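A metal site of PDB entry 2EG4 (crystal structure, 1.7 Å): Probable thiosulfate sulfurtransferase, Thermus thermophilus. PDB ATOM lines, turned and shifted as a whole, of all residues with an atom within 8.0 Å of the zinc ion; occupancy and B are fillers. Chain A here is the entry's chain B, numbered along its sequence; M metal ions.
The backbone NH of Met 218 is in hydrogen-bond range of the backbone carbonyl oxygen of His 192, at 3.5 Å.
Residues that only touch the zinc ion: Pro 149 (3.9 Å). Five residues have an atom within 4 Å of the zinc ion: Pro 149, Cys 151, Cys 152, His 192 and His 219. The nearest printed residue that does not touch the zinc ion is Lys 35 (4.9 Å).
The zinc ion is bound by NE2 of His 192 (2.2 Å), ND1 of His 219 (2.2 Å), SG of Cys 151 (2.3 Å) and SG of Cys 152 (2.3 Å).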
ATOM      1  N   LYS A  35     -31.905 -11.670  24.974  1.00  0.00           N
ATOM      2  CA  LYS A  35     -31.036 -10.958  24.033  1.00  0.00           C
ATOM      3  C   LYS A  35     -30.950  -9.512  24.498  1.00  0.00           C
ATOM      4  O   LYS A  35     -31.961  -8.813  24.589  1.00  0.00           O
ATOM      5  CB  LYS A  35     -31.598 -10.978  22.616  1.00  0.00           C
ATOM      6  CG  LYS A  35     -31.259 -12.209  21.801  1.00  0.00           C
ATOM      7  CD  LYS A  35     -31.734 -12.020  20.363  1.00  0.00           C
ATOM      8  CE  LYS A  35     -31.424 -13.228  19.501  1.00  0.00           C
ATOM      9  NZ  LYS A  35     -32.101 -14.445  20.024  1.00  0.00           N
ATOM     10  N   HIS A 148     -25.824 -17.462   8.047  1.00  0.00           N
ATOM     11  CA  HIS A 148     -26.274 -16.539   9.090  1.00  0.00           C
ATOM     12  C   HIS A 148     -27.625 -16.992   9.604  1.00  0.00           C
ATOM     13  O   HIS A 148     -28.401 -17.611   8.871  1.00  0.00           O
ATOM     14  CB  HIS A 148     -26.386 -15.095   8.548  1.00  0.00           C
ATOM     15  CG  HIS A 148     -27.439 -14.906   7.493  1.00  0.00           C
ATOM     16  ND1 HIS A 148     -27.220 -15.196   6.164  1.00  0.00           N
ATOM     17  CD2 HIS A 148     -28.714 -14.448   7.570  1.00  0.00           C
ATOM     18  CE1 HIS A 148     -28.305 -14.924   5.465  1.00  0.00           C
ATOM     19  NE2 HIS A 148     -29.229 -14.466   6.299  1.00  0.00           N
ATOM     20  N   PRO A 149     -27.927 -16.718  10.892  1.00  0.00           N
ATOM     21  CA  PRO A 149     -29.217 -17.116  11.464  1.00  0.00           C
ATOM     22  C   PRO A 149     -30.314 -16.237  10.841  1.00  0.00           C
ATOM     23  O   PRO A 149     -30.066 -15.111  10.415  1.00  0.00           O
ATOM     24  CB  PRO A 149     -29.020 -16.899  12.976  1.00  0.00           C
ATOM     25  CG  PRO A 149     -27.994 -15.793  13.028  1.00  0.00           C
ATOM     26  CD  PRO A 149     -27.033 -16.117  11.900  1.00  0.00           C
ATOM     27  N   PRO A 150     -31.568 -16.734  10.780  1.00  0.00           N
ATOM     28  CA  PRO A 150     -32.675 -15.986  10.179  1.00  0.00           C
ATOM     29  C   PRO A 150     -33.061 -14.653  10.822  1.00  0.00           C
ATOM     30  O   PRO A 150     -33.737 -13.838  10.197  1.00  0.00           O
ATOM     31  CB  PRO A 150     -33.834 -17.000  10.180  1.00  0.00           C
ATOM     32  CG  PRO A 150     -33.508 -17.927  11.251  1.00  0.00           C
ATOM     33  CD  PRO A 150     -31.997 -18.083  11.193  1.00  0.00           C
ATOM     34  N   CYS A 151     -32.632 -14.450  12.060  1.00  0.00           N
ATOM     35  CA  CYS A 151     -32.920 -13.216  12.795  1.00  0.00           C
ATOM     36  C   CYS A 151     -31.899 -12.122  12.485  1.00  0.00           C
ATOM     37  O   CYS A 151     -32.020 -10.991  12.978  1.00  0.00           O
ATOM     38  CB  CYS A 151     -32.887 -13.505  14.295  1.00  0.00           C
ATOM     39  SG  CYS A 151     -31.312 -14.273  14.793  1.00  0.00           S
ATOM     40  N   CYS A 152     -30.872 -12.476  11.712  1.00  0.00           N
ATOM     41  CA  CYS A 152     -29.820 -11.537  11.290  1.00  0.00           C
ATOM     42  C   CYS A 152     -29.861 -11.278   9.776  1.00  0.00           C
ATOM     43  O   CYS A 152     -30.234 -12.157   8.986  1.00  0.00           O
ATOM     44  CB  CYS A 152     -28.444 -12.055  11.719  1.00  0.00           C
ATOM     45  SG  CYS A 152     -28.087 -11.766  13.478  1.00  0.00           S
ATOM     46  N   PRO A 153     -29.473 -10.066   9.336  1.00  0.00           N
ATOM     47  CA  PRO A 153     -29.489  -9.721   7.904  1.00  0.00           C
ATOM     48  C   PRO A 153     -28.574 -10.423   6.934  1.00  0.00           C
ATOM     49  O   PRO A 153     -28.964 -10.662   5.787  1.00  0.00           O
ATOM     50  CB  PRO A 153     -29.259  -8.216   7.912  1.00  0.00           C
ATOM     51  CG  PRO A 153     -28.361  -8.047   9.120  1.00  0.00           C
ATOM     52  CD  PRO A 153     -29.047  -8.898  10.130  1.00  0.00           C
ATOM     53  N   ARG A 154     -27.366 -10.765   7.371  1.00  0.00           N
ATOM     54  CA  ARG A 154     -26.392 -11.392   6.470  1.00  0.00           C
ATOM     55  C   ARG A 154     -25.288 -12.060   7.269  1.00  0.00           C
ATOM     56  O   ARG A 154     -25.205 -11.874   8.483  1.00  0.00           O
ATOM     57  CB  ARG A 154     -25.768 -10.315   5.588  1.00  0.00           C
ATOM     58  CG  ARG A 154     -24.903  -9.291   6.370  1.00  0.00           C
ATOM     59  CD  ARG A 154     -24.513  -8.097   5.497  1.00  0.00           C
ATOM     60  NE  ARG A 154     -25.708  -7.393   5.038  1.00  0.00           N
ATOM     61  CZ  ARG A 154     -26.414  -6.546   5.767  1.00  0.00           C
ATOM     62  NH1 ARG A 154     -26.058  -6.261   7.021  1.00  0.00           N
ATOM     63  NH2 ARG A 154     -27.521  -6.003   5.250  1.00  0.00           N
ATOM     64  N   HIS A 192     -23.190 -15.405  18.627  1.00  0.00           N
ATOM     65  CA  HIS A 192     -24.387 -14.786  18.071  1.00  0.00           C
ATOM     66  C   HIS A 192     -25.187 -13.961  19.095  1.00  0.00           C
ATOM     67  O   HIS A 192     -25.530 -12.814  18.813  1.00  0.00           O
ATOM     68  CB  HIS A 192     -25.334 -15.816  17.453  1.00  0.00           C
ATOM     69  CG  HIS A 192     -26.664 -15.241  17.058  1.00  0.00           C
ATOM     70  ND1 HIS A 192     -27.834 -15.597  17.693  1.00  0.00           N
ATOM     71  CD2 HIS A 192     -27.001 -14.321  16.119  1.00  0.00           C
ATOM     72  CE1 HIS A 192     -28.837 -14.925  17.156  1.00  0.00           C
ATOM     73  NE2 HIS A 192     -28.352 -14.141  16.197  1.00  0.00           N
ATOM     74  N   SER A 193     -25.465 -14.523  20.260  1.00  0.00           N
ATOM     75  CA  SER A 193     -26.236 -13.788  21.277  1.00  0.00           C
ATOM     76  C   SER A 193     -25.689 -13.998  22.670  1.00  0.00           C
ATOM     77  O   SER A 193     -26.426 -13.844  23.650  1.00  0.00           O
ATOM     78  CB  SER A 193     -27.679 -14.262  21.273  1.00  0.00           C
ATOM     79  OG  SER A 193     -27.763 -15.506  21.940  1.00  0.00           O
ATOM     80  N   GLY A 216     -23.878  -8.831  23.720  1.00  0.00           N
ATOM     81  CA  GLY A 216     -24.639  -8.416  22.562  1.00  0.00           C
ATOM     82  C   GLY A 216     -24.314  -9.277  21.367  1.00  0.00           C
ATOM     83  O   GLY A 216     -25.207  -9.680  20.605  1.00  0.00           O
ATOM     84  N   MET A 218     -22.853 -10.882  17.740  1.00  0.00           N
ATOM     85  CA  MET A 218     -23.204 -10.540  16.370  1.00  0.00           C
ATOM     86  C   MET A 218     -24.633 -10.042  16.154  1.00  0.00           C
ATOM     87  O   MET A 218     -24.884  -9.179  15.315  1.00  0.00           O
ATOM     88  CB  MET A 218     -22.952 -11.721  15.412  1.00  0.00           C
ATOM     89  CG  MET A 218     -21.501 -11.972  15.078  1.00  0.00           C
ATOM     90  SD  MET A 218     -20.592 -10.536  14.446  1.00  0.00           S
ATOM     91  CE  MET A 218     -21.303 -10.206  12.946  1.00  0.00           C
ATOM     92  N   HIS A 219     -25.576 -10.581  16.919  1.00  0.00           N
ATOM     93  CA  HIS A 219     -26.945 -10.127  16.747  1.00  0.00           C
ATOM     94  C   HIS A 219     -27.033  -8.625  17.006  1.00  0.00           C
ATOM     95  O   HIS A 219     -27.587  -7.884  16.202  1.00  0.00           O
ATOM     96  CB  HIS A 219     -27.897 -10.855  17.687  1.00  0.00           C
ATOM     97  CG  HIS A 219     -29.334 -10.572  17.377  1.00  0.00           C
ATOM     98  ND1 HIS A 219     -29.984 -11.138  16.307  1.00  0.00           N
ATOM     99  CD2 HIS A 219     -30.203  -9.701  17.933  1.00  0.00           C
ATOM    100  CE1 HIS A 219     -31.194 -10.632  16.206  1.00  0.00           C
ATOM    101  NE2 HIS A 219     -31.362  -9.755  17.182  1.00  0.00           N
ATOM    102  N   GLU A 220     -26.469  -8.169  18.113  1.00  0.00           N
ATOM    103  CA  GLU A 220     -26.525  -6.729  18.399  1.00  0.00           C
ATOM    104  C   GLU A 220     -25.681  -5.954  17.403  1.00  0.00           C
ATOM    105  O   GLU A 220     -26.096  -4.902  16.893  1.00  0.00           O
ATOM    106  CB  GLU A 220     -26.024  -6.427  19.823  1.00  0.00           C
ATOM    107  CG  GLU A 220     -26.052  -4.929  20.128  1.00  0.00           C
ATOM    108  CD  GLU A 220     -25.366  -4.598  21.435  1.00  0.00           C
ATOM    109  OE1 GLU A 220     -24.240  -5.075  21.629  1.00  0.00           O
ATOM    110  OE2 GLU A 220     -25.964  -3.859  22.247  1.00  0.00           O
ATOM    111  N   LEU A 222     -25.009  -6.490  14.339  1.00  0.00           N
ATOM    112  CA  LEU A 222     -25.704  -6.293  13.085  1.00  0.00           C
ATOM    113  C   LEU A 222     -26.926  -5.389  13.236  1.00  0.00           C
ATOM    114  O   LEU A 222     -27.249  -4.621  12.334  1.00  0.00           O
ATOM    115  CB  LEU A 222     -26.101  -7.641  12.475  1.00  0.00           C
ATOM    116  CG  LEU A 222     -24.882  -8.351  11.868  1.00  0.00           C
ATOM    117  CD1 LEU A 222     -25.244  -9.794  11.521  1.00  0.00           C
ATOM    118  CD2 LEU A 222     -24.413  -7.582  10.635  1.00  0.00           C
ATOM    119  N   GLN A 223     -27.619  -5.485  14.370  1.00  0.00           N
ATOM    120  CA  GLN A 223     -28.785  -4.646  14.573  1.00  0.00           C
ATOM    121  C   GLN A 223     -28.313  -3.192  14.639  1.00  0.00           C
ATOM    122  O   GLN A 223     -29.032  -2.295  14.202  1.00  0.00           O
ATOM    123  CB  GLN A 223     -29.530  -5.019  15.869  1.00  0.00           C
ATOM    124  CG  GLN A 223     -30.372  -6.288  15.751  1.00  0.00           C
ATOM    125  CD  GLN A 223     -31.349  -6.255  14.564  1.00  0.00           C
ATOM    126  OE1 GLN A 223     -32.058  -5.270  14.360  1.00  0.00           O
ATOM    127  NE2 GLN A 223     -31.371  -7.346  13.780  1.00  0.00           N
HETATM  128 ZN    ZN M   1     -29.553 -12.807  14.990  1.00  0.00          ZN
